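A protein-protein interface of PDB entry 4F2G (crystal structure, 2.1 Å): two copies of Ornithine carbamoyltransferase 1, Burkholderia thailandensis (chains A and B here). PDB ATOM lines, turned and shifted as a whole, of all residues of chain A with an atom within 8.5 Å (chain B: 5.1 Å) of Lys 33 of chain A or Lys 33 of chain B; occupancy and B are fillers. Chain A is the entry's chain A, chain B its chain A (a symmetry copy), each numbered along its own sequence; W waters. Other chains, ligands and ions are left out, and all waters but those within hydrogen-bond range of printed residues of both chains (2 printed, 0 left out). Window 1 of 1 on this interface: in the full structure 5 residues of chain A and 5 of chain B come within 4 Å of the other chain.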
ATOM      1  N   ARG A  26     -14.294  23.887 -18.663  1.00  0.00           N
ATOM      2  CA  ARG A  26     -15.459  24.718 -19.000  1.00  0.00           C
ATOM      3  C   ARG A  26     -15.028  26.065 -19.557  1.00  0.00           C
ATOM      4  O   ARG A  26     -15.645  26.569 -20.483  1.00  0.00           O
ATOM      5  CB  ARG A  26     -16.383  24.955 -17.794  1.00  0.00           C
ATOM      6  CG  ARG A  26     -17.264  23.779 -17.427  1.00  0.00           C
ATOM      7  CD  ARG A  26     -17.956  23.188 -18.649  1.00  0.00           C
ATOM      8  NE  ARG A  26     -19.153  23.928 -19.041  1.00  0.00           N
ATOM      9  CZ  ARG A  26     -19.888  23.626 -20.106  1.00  0.00           C
ATOM     10  NH1 ARG A  26     -19.540  22.609 -20.884  1.00  0.00           N
ATOM     11  NH2 ARG A  26     -20.967  24.339 -20.395  1.00  0.00           N
ATOM     12  N   THR A  27     -13.985  26.655 -18.977  1.00  0.00           N
ATOM     13  CA  THR A  27     -13.497  27.953 -19.438  1.00  0.00           C
ATOM     14  C   THR A  27     -13.158  27.903 -20.928  1.00  0.00           C
ATOM     15  O   THR A  27     -13.544  28.784 -21.700  1.00  0.00           O
ATOM     16  CB  THR A  27     -12.260  28.430 -18.634  1.00  0.00           C
ATOM     17  OG1 THR A  27     -12.634  28.647 -17.264  1.00  0.00           O
ATOM     18  CG2 THR A  27     -11.725  29.735 -19.216  1.00  0.00           C
ATOM     19  N   GLY A  28     -12.441  26.861 -21.330  1.00  0.00           N
ATOM     20  CA  GLY A  28     -12.061  26.697 -22.722  1.00  0.00           C
ATOM     21  C   GLY A  28     -13.271  26.457 -23.600  1.00  0.00           C
ATOM     22  O   GLY A  28     -13.361  26.986 -24.697  1.00  0.00           O
ATOM     23  N   ILE A  29     -14.206  25.648 -23.117  1.00  0.00           N
ATOM     24  CA  ILE A  29     -15.436  25.386 -23.855  1.00  0.00           C
ATOM     25  C   ILE A  29     -16.286  26.659 -24.053  1.00  0.00           C
ATOM     26  O   ILE A  29     -16.748  26.945 -25.156  1.00  0.00           O
ATOM     27  CB  ILE A  29     -16.264  24.286 -23.153  1.00  0.00           C
ATOM     28  CG1 ILE A  29     -15.534  22.945 -23.243  1.00  0.00           C
ATOM     29  CG2 ILE A  29     -17.667  24.192 -23.743  1.00  0.00           C
ATOM     30  CD1 ILE A  29     -16.069  21.899 -22.290  1.00  0.00           C
ATOM     31  N   LEU A  30     -16.485  27.428 -22.989  1.00  0.00           N
ATOM     32  CA  LEU A  30     -17.294  28.635 -23.080  1.00  0.00           C
ATOM     33  C   LEU A  30     -16.602  29.705 -23.923  1.00  0.00           C
ATOM     34  O   LEU A  30     -17.261  30.494 -24.601  1.00  0.00           O
ATOM     35  CB  LEU A  30     -17.608  29.185 -21.689  1.00  0.00           C
ATOM     36  CG  LEU A  30     -18.406  28.308 -20.719  1.00  0.00           C
ATOM     37  CD1 LEU A  30     -18.627  29.053 -19.420  1.00  0.00           C
ATOM     38  CD2 LEU A  30     -19.734  27.892 -21.317  1.00  0.00           C
ATOM     39  N   LYS A  31     -15.272  29.736 -23.876  1.00  0.00           N
ATOM     40  CA  LYS A  31     -14.514  30.686 -24.684  1.00  0.00           C
ATOM     41  C   LYS A  31     -14.694  30.372 -26.169  1.00  0.00           C
ATOM     42  O   LYS A  31     -14.823  31.283 -26.993  1.00  0.00           O
ATOM     43  CB  LYS A  31     -13.031  30.692 -24.298  1.00  0.00           C
ATOM     44  CG  LYS A  31     -12.203  31.776 -25.008  1.00  0.00           C
ATOM     45  CD  LYS A  31     -10.803  31.888 -24.413  1.00  0.00           C
ATOM     46  CE  LYS A  31      -9.949  32.898 -25.158  1.00  0.00           C
ATOM     47  NZ  LYS A  31      -8.635  33.099 -24.488  1.00  0.00           N
ATOM     48  N   ARG A  32     -14.718  29.079 -26.502  1.00  0.00           N
ATOM     49  CA  ARG A  32     -14.950  28.637 -27.878  1.00  0.00           C
ATOM     50  C   ARG A  32     -16.352  29.008 -28.367  1.00  0.00           C
ATOM     51  O   ARG A  32     -16.526  29.418 -29.521  1.00  0.00           O
ATOM     52  CB  ARG A  32     -14.684  27.137 -28.043  1.00  0.00           C
ATOM     53  CG  ARG A  32     -13.201  26.796 -28.051  1.00  0.00           C
ATOM     54  CD  ARG A  32     -12.941  25.289 -28.070  1.00  0.00           C
ATOM     55  NE  ARG A  32     -11.705  24.962 -27.352  1.00  0.00           N
ATOM     56  CZ  ARG A  32     -11.652  24.313 -26.187  1.00  0.00           C
ATOM     57  NH1 ARG A  32     -12.769  23.889 -25.604  1.00  0.00           N
ATOM     58  NH2 ARG A  32     -10.478  24.075 -25.608  1.00  0.00           N
ATOM     59  N   LYS A  33     -17.343  28.879 -27.486  1.00  0.00           N
ATOM     60  CA  LYS A  33     -18.703  29.322 -27.787  1.00  0.00           C
ATOM     61  C   LYS A  33     -18.748  30.835 -27.996  1.00  0.00           C
ATOM     62  O   LYS A  33     -19.407  31.328 -28.912  1.00  0.00           O
ATOM     63  CB  LYS A  33     -19.660  28.914 -26.666  1.00  0.00           C
ATOM     64  CG  LYS A  33     -19.982  27.429 -26.635  1.00  0.00           C
ATOM     65  CD  LYS A  33     -21.158  27.138 -25.718  1.00  0.00           C
ATOM     66  CE  LYS A  33     -20.832  26.021 -24.740  1.00  0.00           C
ATOM     67  NZ  LYS A  33     -21.810  24.901 -24.829  1.00  0.00           N
ATOM     68  N   PHE A  34     -18.033  31.564 -27.143  1.00  0.00           N
ATOM     69  CA  PHE A  34     -17.839  33.004 -27.308  1.00  0.00           C
ATOM     70  C   PHE A  34     -17.238  33.294 -28.690  1.00  0.00           C
ATOM     71  O   PHE A  34     -17.783  34.088 -29.453  1.00  0.00           O
ATOM     72  CB  PHE A  34     -16.949  33.542 -26.166  1.00  0.00           C
ATOM     73  CG  PHE A  34     -16.562  35.010 -26.294  1.00  0.00           C
ATOM     74  CD1 PHE A  34     -17.485  36.019 -26.050  1.00  0.00           C
ATOM     75  CD2 PHE A  34     -15.253  35.375 -26.617  1.00  0.00           C
ATOM     76  CE1 PHE A  34     -17.120  37.365 -26.154  1.00  0.00           C
ATOM     77  CE2 PHE A  34     -14.883  36.720 -26.721  1.00  0.00           C
ATOM     78  CZ  PHE A  34     -15.819  37.713 -26.488  1.00  0.00           C
ATOM     79  N   LYS A  35     -16.136  32.633 -29.033  1.00  0.00           N
ATOM     80  CA  LYS A  35     -15.484  32.912 -30.315  1.00  0.00           C
ATOM     81  C   LYS A  35     -16.286  32.392 -31.507  1.00  0.00           C
ATOM     82  O   LYS A  35     -16.095  32.855 -32.623  1.00  0.00           O
ATOM     83  CB  LYS A  35     -14.030  32.409 -30.339  1.00  0.00           C
ATOM     84  N   ASN A  36     -17.201  31.453 -31.278  1.00  0.00           N
ATOM     85  CA  ASN A  36     -18.074  30.950 -32.356  1.00  0.00           C
ATOM     86  C   ASN A  36     -19.428  31.692 -32.485  1.00  0.00           C
ATOM     87  O   ASN A  36     -20.276  31.311 -33.301  1.00  0.00           O
ATOM     88  CB  ASN A  36     -18.342  29.442 -32.200  1.00  0.00           C
ATOM     89  CG  ASN A  36     -17.167  28.574 -32.630  1.00  0.00           C
ATOM     90  OD1 ASN A  36     -16.503  28.850 -33.624  1.00  0.00           O
ATOM     91  ND2 ASN A  36     -16.928  27.496 -31.888  1.00  0.00           N
ATOM     92  N   TYR A  37     -19.631  32.733 -31.674  1.00  0.00           N
ATOM     93  CA  TYR A  37     -20.894  33.480 -31.676  1.00  0.00           C
ATOM     94  C   TYR A  37     -22.064  32.502 -31.531  1.00  0.00           C
ATOM     95  O   TYR A  37     -23.095  32.623 -32.195  1.00  0.00           O
ATOM     96  CB  TYR A  37     -21.030  34.321 -32.959  1.00  0.00           C
ATOM     97  N   GLU A  38     -21.880  31.514 -30.666  1.00  0.00           N
ATOM     98  CA  GLU A  38     -22.919  30.543 -30.381  1.00  0.00           C
ATOM     99  C   GLU A  38     -23.747  31.072 -29.210  1.00  0.00           C
ATOM    100  O   GLU A  38     -23.197  31.535 -28.212  1.00  0.00           O
ATOM    101  CB  GLU A  38     -22.276  29.202 -30.038  1.00  0.00           C
ATOM    102  CG  GLU A  38     -23.235  28.124 -29.584  1.00  0.00           C
ATOM    103  CD  GLU A  38     -22.523  26.813 -29.267  1.00  0.00           C
ATOM    104  OE1 GLU A  38     -21.886  26.236 -30.180  1.00  0.00           O
ATOM    105  OE2 GLU A  38     -22.603  26.364 -28.099  1.00  0.00           O
ATOM    106  N   THR A  39     -25.068  31.034 -29.338  1.00  0.00           N
ATOM    107  CA  THR A  39     -25.930  31.514 -28.261  1.00  0.00           C
ATOM    108  C   THR A  39     -26.068  30.461 -27.161  1.00  0.00           C
ATOM    109  O   THR A  39     -26.595  29.365 -27.394  1.00  0.00           O
ATOM    110  CB  THR A  39     -27.331  31.880 -28.774  1.00  0.00           C
ATOM    111  OG1 THR A  39     -27.216  32.836 -29.827  1.00  0.00           O
ATOM    112  CG2 THR A  39     -28.162  32.478 -27.649  1.00  0.00           C
ATOM    113  N   TYR A  40     -25.571  30.794 -25.975  1.00  0.00           N
ATOM    114  CA  TYR A  40     -25.644  29.906 -24.822  1.00  0.00           C
ATOM    115  C   TYR A  40     -26.034  30.717 -23.597  1.00  0.00           C
ATOM    116  O   TYR A  40     -25.266  31.561 -23.130  1.00  0.00           O
ATOM    117  CB  TYR A  40     -24.302  29.209 -24.592  1.00  0.00           C
ATOM    118  CG  TYR A  40     -24.289  28.287 -23.394  1.00  0.00           C
ATOM    119  CD1 TYR A  40     -25.216  27.261 -23.272  1.00  0.00           C
ATOM    120  CD2 TYR A  40     -23.347  28.441 -22.384  1.00  0.00           C
ATOM    121  CE1 TYR A  40     -25.208  26.416 -22.180  1.00  0.00           C
ATOM    122  CE2 TYR A  40     -23.331  27.601 -21.289  1.00  0.00           C
ATOM    123  CZ  TYR A  40     -24.263  26.590 -21.191  1.00  0.00           C
ATOM    124  OH  TYR A  40     -24.250  25.750 -20.101  1.00  0.00           O
ATOM    125  N   HIS A  41     -27.232  30.470 -23.082  1.00  0.00           N
ATOM    126  CA  HIS A  41     -27.769  31.275 -21.983  1.00  0.00           C
ATOM    127  C   HIS A  41     -28.243  30.452 -20.796  1.00  0.00           C
ATOM    128  O   HIS A  41     -29.425  30.510 -20.454  1.00  0.00           O
ATOM    129  CB  HIS A  41     -28.967  32.084 -22.461  1.00  0.00           C
ATOM    130  CG  HIS A  41     -28.639  33.109 -23.495  1.00  0.00           C
ATOM    131  ND1 HIS A  41     -27.379  33.648 -23.636  1.00  0.00           N
ATOM    132  CD2 HIS A  41     -29.410  33.698 -24.435  1.00  0.00           C
ATOM    133  CE1 HIS A  41     -27.388  34.525 -24.621  1.00  0.00           C
ATOM    134  NE2 HIS A  41     -28.607  34.573 -25.126  1.00  0.00           N
ATOM    135  N   PRO A  42     -27.364  29.728 -20.165  1.00  0.00           N
ATOM    136  CA  PRO A  42     -27.754  28.938 -19.019  1.00  0.00           C
ATOM    137  C   PRO A  42     -28.175  29.756 -17.830  1.00  0.00           C
ATOM    138  O   PRO A  42     -28.876  29.289 -17.013  1.00  0.00           O
ATOM    139  CB  PRO A  42     -26.512  28.136 -18.734  1.00  0.00           C
ATOM    140  CG  PRO A  42     -25.460  29.044 -19.112  1.00  0.00           C
ATOM    141  CD  PRO A  42     -25.945  29.609 -20.398  1.00  0.00           C
ATOM    142  N   GLN A  69     -23.395  37.553 -21.482  1.00  0.00           N
ATOM    143  CA  GLN A  69     -23.138  36.523 -22.481  1.00  0.00           C
ATOM    144  C   GLN A  69     -23.703  35.174 -22.064  1.00  0.00           C
ATOM    145  O   GLN A  69     -23.901  34.313 -22.906  1.00  0.00           O
ATOM    146  CB  GLN A  69     -21.635  36.405 -22.766  1.00  0.00           C
ATOM    147  CG  GLN A  69     -21.027  37.693 -23.316  1.00  0.00           C
ATOM    148  CD  GLN A  69     -19.509  37.698 -23.273  1.00  0.00           C
ATOM    149  OE1 GLN A  69     -18.886  36.750 -22.790  1.00  0.00           O
ATOM    150  NE2 GLN A  69     -18.906  38.771 -23.782  1.00  0.00           N
ATOM    151  N   LEU A  70     -23.962  34.995 -20.768  1.00  0.00           N
ATOM    152  CA  LEU A  70     -24.582  33.762 -20.272  1.00  0.00           C
ATOM    153  C   LEU A  70     -26.103  33.905 -20.107  1.00  0.00           C
ATOM    154  O   LEU A  70     -26.769  32.987 -19.636  1.00  0.00           O
ATOM    155  CB  LEU A  70     -23.933  33.312 -18.955  1.00  0.00           C
ATOM    156  CG  LEU A  70     -22.461  32.878 -19.024  1.00  0.00           C
ATOM    157  CD1 LEU A  70     -21.939  32.489 -17.640  1.00  0.00           C
ATOM    158  CD2 LEU A  70     -22.267  31.733 -20.025  1.00  0.00           C
ATOM    159  N   HIS A 293     -13.421  34.999 -19.220  1.00  0.00           N
ATOM    160  CA  HIS A 293     -13.753  33.613 -19.516  1.00  0.00           C
ATOM    161  C   HIS A 293     -13.757  32.711 -18.291  1.00  0.00           C
ATOM    162  O   HIS A 293     -14.656  31.880 -18.152  1.00  0.00           O
ATOM    163  CB  HIS A 293     -12.878  33.069 -20.659  1.00  0.00           C
ATOM    164  CG  HIS A 293     -12.915  33.937 -21.877  1.00  0.00           C
ATOM    165  ND1 HIS A 293     -14.058  34.108 -22.627  1.00  0.00           N
ATOM    166  CD2 HIS A 293     -11.975  34.736 -22.434  1.00  0.00           C
ATOM    167  CE1 HIS A 293     -13.812  34.950 -23.614  1.00  0.00           C
ATOM    168  NE2 HIS A 293     -12.555  35.348 -23.520  1.00  0.00           N
ATOM    169  N   LYS A 296     -16.880  33.534 -16.169  1.00  0.00           N
ATOM    170  CA  LYS A 296     -18.093  32.928 -16.711  1.00  0.00           C
ATOM    171  C   LYS A 296     -18.181  31.462 -16.283  1.00  0.00           C
ATOM    172  O   LYS A 296     -19.239  30.990 -15.872  1.00  0.00           O
ATOM    173  CB  LYS A 296     -18.135  33.049 -18.238  1.00  0.00           C
ATOM    174  CG  LYS A 296     -18.465  34.465 -18.739  1.00  0.00           C
ATOM    175  CD  LYS A 296     -18.210  34.628 -20.241  1.00  0.00           C
ATOM    176  CE  LYS A 296     -19.241  33.877 -21.073  1.00  0.00           C
ATOM    177  NZ  LYS A 296     -18.926  33.981 -22.531  1.00  0.00           N
ATOM    178  N   GLU A 300     -21.160  29.891 -13.907  1.00  0.00           N
ATOM    179  CA  GLU A 300     -21.891  28.727 -14.379  1.00  0.00           C
ATOM    180  C   GLU A 300     -21.777  27.599 -13.351  1.00  0.00           C
ATOM    181  O   GLU A 300     -22.767  26.968 -12.984  1.00  0.00           O
ATOM    182  CB  GLU A 300     -21.326  28.266 -15.725  1.00  0.00           C
ATOM    183  CG  GLU A 300     -22.234  27.325 -16.488  1.00  0.00           C
ATOM    184  CD  GLU A 300     -21.494  26.588 -17.582  1.00  0.00           C
ATOM    185  OE1 GLU A 300     -20.431  26.005 -17.289  1.00  0.00           O
ATOM    186  OE2 GLU A 300     -21.962  26.600 -18.737  1.00  0.00           O
ATOM    187  N   LEU A 307     -22.112  19.809 -15.378  1.00  0.00           N
ATOM    188  CA  LEU A 307     -23.093  19.355 -16.336  1.00  0.00           C
ATOM    189  C   LEU A 307     -23.427  17.861 -16.226  1.00  0.00           C
ATOM    190  O   LEU A 307     -22.779  17.124 -15.506  1.00  0.00           O
ATOM    191  CB  LEU A 307     -22.703  19.747 -17.765  1.00  0.00           C
ATOM    192  N   ARG B  26     -19.380  15.287 -32.721  1.00  0.00           N
ATOM    193  CA  ARG B  26     -20.538  16.185 -32.601  1.00  0.00           C
ATOM    194  C   ARG B  26     -21.765  15.429 -32.118  1.00  0.00           C
ATOM    195  O   ARG B  26     -22.530  15.953 -31.320  1.00  0.00           O
ATOM    196  CB  ARG B  26     -20.880  16.889 -33.924  1.00  0.00           C
ATOM    197  CG  ARG B  26     -19.964  18.038 -34.288  1.00  0.00           C
ATOM    198  CD  ARG B  26     -19.739  18.977 -33.110  1.00  0.00           C
ATOM    199  NE  ARG B  26     -20.829  19.935 -32.930  1.00  0.00           N
ATOM    200  CZ  ARG B  26     -20.874  20.818 -31.938  1.00  0.00           C
ATOM    201  NH1 ARG B  26     -19.901  20.853 -31.037  1.00  0.00           N
ATOM    202  NH2 ARG B  26     -21.891  21.663 -31.843  1.00  0.00           N
ATOM    203  N   ILE B  29     -21.563  15.084 -28.462  1.00  0.00           N
ATOM    204  CA  ILE B  29     -21.747  16.398 -27.856  1.00  0.00           C
ATOM    205  C   ILE B  29     -23.221  16.852 -27.875  1.00  0.00           C
ATOM    206  O   ILE B  29     -23.753  17.306 -26.864  1.00  0.00           O
ATOM    207  CB  ILE B  29     -20.848  17.445 -28.552  1.00  0.00           C
ATOM    208  CG1 ILE B  29     -19.376  17.149 -28.256  1.00  0.00           C
ATOM    209  CG2 ILE B  29     -21.224  18.861 -28.126  1.00  0.00           C
ATOM    210  CD1 ILE B  29     -18.417  17.880 -29.169  1.00  0.00           C
ATOM    211  N   LEU B  30     -23.882  16.722 -29.019  1.00  0.00           N
ATOM    212  CA  LEU B  30     -25.269  17.149 -29.131  1.00  0.00           C
ATOM    213  C   LEU B  30     -26.194  16.252 -28.311  1.00  0.00           C
ATOM    214  O   LEU B  30     -27.212  16.710 -27.788  1.00  0.00           O
ATOM    215  CB  LEU B  30     -25.715  17.164 -30.594  1.00  0.00           C
ATOM    216  CG  LEU B  30     -24.990  18.094 -31.569  1.00  0.00           C
ATOM    217  CD1 LEU B  30     -25.607  17.971 -32.948  1.00  0.00           C
ATOM    218  CD2 LEU B  30     -25.038  19.533 -31.099  1.00  0.00           C
ATOM    219  N   LYS B  31     -25.845  14.973 -28.201  1.00  0.00           N
ATOM    220  CA  LYS B  31     -26.633  14.045 -27.396  1.00  0.00           C
ATOM    221  C   LYS B  31     -26.561  14.439 -25.921  1.00  0.00           C
ATOM    222  O   LYS B  31     -27.564  14.368 -25.203  1.00  0.00           O
ATOM    223  CB  LYS B  31     -26.176  12.595 -27.601  1.00  0.00           C
ATOM    224  CG  LYS B  31     -27.060  11.554 -26.896  1.00  0.00           C
ATOM    225  CD  LYS B  31     -26.703  10.137 -27.328  1.00  0.00           C
ATOM    226  CE  LYS B  31     -27.513   9.093 -26.578  1.00  0.00           C
ATOM    227  NZ  LYS B  31     -27.255   7.724 -27.103  1.00  0.00           N
ATOM    228  N   ARG B  32     -25.378  14.869 -25.480  1.00  0.00           N
ATOM    229  CA  ARG B  32     -25.185  15.342 -24.107  1.00  0.00           C
ATOM    230  C   ARG B  32     -25.989  16.611 -23.824  1.00  0.00           C
ATOM    231  O   ARG B  32     -26.567  16.758 -22.740  1.00  0.00           O
ATOM    232  CB  ARG B  32     -23.702  15.540 -23.779  1.00  0.00           C
ATOM    233  CG  ARG B  32     -22.962  14.229 -23.564  1.00  0.00           C
ATOM    234  CD  ARG B  32     -21.455  14.423 -23.382  1.00  0.00           C
ATOM    235  NE  ARG B  32     -20.712  13.278 -23.915  1.00  0.00           N
ATOM    236  CZ  ARG B  32     -19.939  13.313 -25.004  1.00  0.00           C
ATOM    237  NH1 ARG B  32     -19.780  14.449 -25.677  1.00  0.00           N
ATOM    238  NH2 ARG B  32     -19.314  12.213 -25.414  1.00  0.00           N
ATOM    239  N   LYS B  33     -26.041  17.515 -24.802  1.00  0.00           N
ATOM    240  CA  LYS B  33     -26.881  18.706 -24.706  1.00  0.00           C
ATOM    241  C   LYS B  33     -28.361  18.327 -24.639  1.00  0.00           C
ATOM    242  O   LYS B  33     -29.124  18.891 -23.855  1.00  0.00           O
ATOM    243  CB  LYS B  33     -26.628  19.637 -25.891  1.00  0.00           C
ATOM    244  CG  LYS B  33     -25.300  20.375 -25.830  1.00  0.00           C
ATOM    245  CD  LYS B  33     -25.243  21.499 -26.851  1.00  0.00           C
ATOM    246  CE  LYS B  33     -23.972  21.428 -27.680  1.00  0.00           C
ATOM    247  NZ  LYS B  33     -23.191  22.695 -27.610  1.00  0.00           N
ATOM    248  N   PHE B  34     -28.752  17.356 -25.461  1.00  0.00           N
ATOM    249  CA  PHE B  34     -30.086  16.767 -25.403  1.00  0.00           C
ATOM    250  C   PHE B  34     -30.359  16.233 -23.989  1.00  0.00           C
ATOM    251  O   PHE B  34     -31.359  16.586 -23.371  1.00  0.00           O
ATOM    252  CB  PHE B  34     -30.213  15.661 -26.474  1.00  0.00           C
ATOM    253  CG  PHE B  34     -31.518  14.874 -26.431  1.00  0.00           C
ATOM    254  CD1 PHE B  34     -32.709  15.437 -26.871  1.00  0.00           C
ATOM    255  CD2 PHE B  34     -31.537  13.551 -25.988  1.00  0.00           C
ATOM    256  CE1 PHE B  34     -33.901  14.706 -26.844  1.00  0.00           C
ATOM    257  CE2 PHE B  34     -32.726  12.813 -25.961  1.00  0.00           C
ATOM    258  CZ  PHE B  34     -33.906  13.395 -26.390  1.00  0.00           C
ATOM    259  N   LYS B  35     -29.462  15.405 -23.462  1.00  0.00           N
ATOM    260  CA  LYS B  35     -29.696  14.817 -22.140  1.00  0.00           C
ATOM    261  C   LYS B  35     -29.569  15.838 -21.010  1.00  0.00           C
ATOM    262  O   LYS B  35     -30.090  15.620 -19.925  1.00  0.00           O
ATOM    263  CB  LYS B  35     -28.812  13.581 -21.899  1.00  0.00           C
ATOM    264  N   ASN B  36     -28.904  16.963 -21.263  1.00  0.00           N
ATOM    265  CA  ASN B  36     -28.799  18.037 -20.257  1.00  0.00           C
ATOM    266  C   ASN B  36     -29.901  19.122 -20.357  1.00  0.00           C
ATOM    267  O   ASN B  36     -29.874  20.113 -19.617  1.00  0.00           O
ATOM    268  CB  ASN B  36     -27.421  18.719 -20.308  1.00  0.00           C
ATOM    269  CG  ASN B  36     -26.315  17.892 -19.667  1.00  0.00           C
ATOM    270  OD1 ASN B  36     -26.509  17.268 -18.629  1.00  0.00           O
ATOM    271  ND2 ASN B  36     -25.132  17.913 -20.277  1.00  0.00           N
ATOM    272  N   TYR B  37     -30.854  18.939 -21.274  1.00  0.00           N
ATOM    273  CA  TYR B  37     -31.921  19.923 -21.490  1.00  0.00           C
ATOM    274  C   TYR B  37     -31.301  21.310 -21.686  1.00  0.00           C
ATOM    275  O   TYR B  37     -31.784  22.315 -21.162  1.00  0.00           O
ATOM    276  CB  TYR B  37     -32.912  19.922 -20.312  1.00  0.00           C
ATOM    277  N   GLU B  38     -30.204  21.348 -22.433  1.00  0.00           N
ATOM    278  CA  GLU B  38     -29.537  22.595 -22.751  1.00  0.00           C
ATOM    279  C   GLU B  38     -30.135  23.125 -24.054  1.00  0.00           C
ATOM    280  O   GLU B  38     -30.302  22.378 -25.017  1.00  0.00           O
ATOM    281  CB  GLU B  38     -28.039  22.345 -22.895  1.00  0.00           C
ATOM    282  CG  GLU B  38     -27.227  23.531 -23.364  1.00  0.00           C
ATOM    283  CD  GLU B  38     -25.741  23.208 -23.476  1.00  0.00           C
ATOM    284  OE1 GLU B  38     -25.122  22.851 -22.444  1.00  0.00           O
ATOM    285  OE2 GLU B  38     -25.197  23.312 -24.601  1.00  0.00           O
ATOM    286  N   TYR B  40     -29.996  24.656 -27.446  1.00  0.00           N
ATOM    287  CA  TYR B  40     -29.034  24.883 -28.517  1.00  0.00           C
ATOM    288  C   TYR B  40     -29.770  24.910 -29.847  1.00  0.00           C
ATOM    289  O   TYR B  40     -30.301  23.891 -30.292  1.00  0.00           O
ATOM    290  CB  TYR B  40     -27.966  23.788 -28.521  1.00  0.00           C
ATOM    291  CG  TYR B  40     -26.941  23.940 -29.623  1.00  0.00           C
ATOM    292  CD1 TYR B  40     -26.211  25.111 -29.765  1.00  0.00           C
ATOM    293  CD2 TYR B  40     -26.704  22.908 -30.523  1.00  0.00           C
ATOM    294  CE1 TYR B  40     -25.274  25.254 -30.769  1.00  0.00           C
ATOM    295  CE2 TYR B  40     -25.768  23.042 -31.532  1.00  0.00           C
ATOM    296  CZ  TYR B  40     -25.056  24.215 -31.649  1.00  0.00           C
ATOM    297  OH  TYR B  40     -24.121  24.352 -32.651  1.00  0.00           O
HETATM  298  O   HOH W   1     -25.987  24.022 -19.942  1.00  0.00           O
HETATM  299  O   HOH W   2     -22.946  26.497 -32.862  1.00  0.00           O
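The side-chain amino group (NZ) of Lys 33 of chain A is in salt-bridge range of the side-chain carboxylate (OE2) of Glu 38 of chain B. The side-chain carboxylate (OE2) of Glu 38 of chain A lies within salt-bridge range of the side-chain amino group (NZ) of Lys 33 of chain B (3.7 Å).
NZ of Lys 33 of chain A lies within salt-bridge range of OE2 of Glu 38 of chain A, at 3.7 Å. The side-chain hydroxyl (OH) of Tyr 40 of chain A sits at hydrogen-bond distance from the side-chain carboxylate (OE2) of Glu 300 of chain A. O of Arg 32 of chain B lies within hydrogen-bond range of ND2 of Asn 36 of chain B (3.1 Å). The side-chain carboxylate (OE2) of Glu 38 of chain B is in salt-bridge range of the side-chain amino group (NZ) of Lys 33 of chain B.
Lys 33 of chain B touches Lys 33 of chain A. Glu 38 of chain A touches Tyr 40 of chain B. Glu 38 of chain B touches Tyr 40 of chain A. Leu 307 of chain A touches Asn 36 of chain B.
Of chain B, only Lys 33 (3.8 Å) and Glu 38 (3.7 Å) come within 4 Å of Lys 33 of chain A. Of the printed residues of chain B, Glu 38 of chain A touches Lys 33 (3.7 Å) and Tyr 40 (3.5 Å). Printed residues of chain B within 4 Å of Tyr 40 of chain A: Glu 38 (3.5 Å). Leu 70 of chain A touches none of the printed residues of chain B. Of the printed residues of chain A, Lys 33 of chain B touches Lys 33 and Glu 38. Lys 35 of chain B touches none of the printed residues of chain A. Of the printed residues of chain A, Asn 36 of chain B touches Leu 307. Glu 38 of chain B touches just these residues of chain A: Lys 33 and Tyr 40. The nearest printed residue of chain B that does not touch Lys 33 of chain A is Tyr 40 of chain B (6.6 Å). The nearest residue of chain A that does not touch Lys 33 of chain B is Tyr 40 of chain A (6.6 Å).
Printed residues of chain B that touch a printed residue of chain A: Lys 33, Asn 36, Glu 38 and Tyr 40. Hydrophobic or aromatic side chains of chain B that line the printed part of chain A: Tyr 40. Printed residues of chain A that touch a printed residue of chain B: Lys 33, Glu 38, Tyr 40 and Leu 307.
Lys 33 of chain B touches its own counterpart, Lys 33 of chain A. Lys 33 of chain A touches Glu 38 of chain B, and with the chains exchanged Glu 38 of chain A touches Lys 33 of chain B. Glu 38 of chain A touches Tyr 40 of chain B, and with the chains exchanged Tyr 40 of chain A touches Glu 38 of chain B. Of the 6 pairs that touch across the chains among the printed residues, 5 have their exchanged pair printed and touching as well.
Water W2 bridges the side-chain hydroxyl (OH) of Tyr 40 of chain B and the side-chain carboxylate (OE1) of Glu 38 of chain A. Water W1 bridges OH of Tyr 40 of chain A (2.5 Å) and OE1 of Glu 38 of chain B (2.9 Å).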
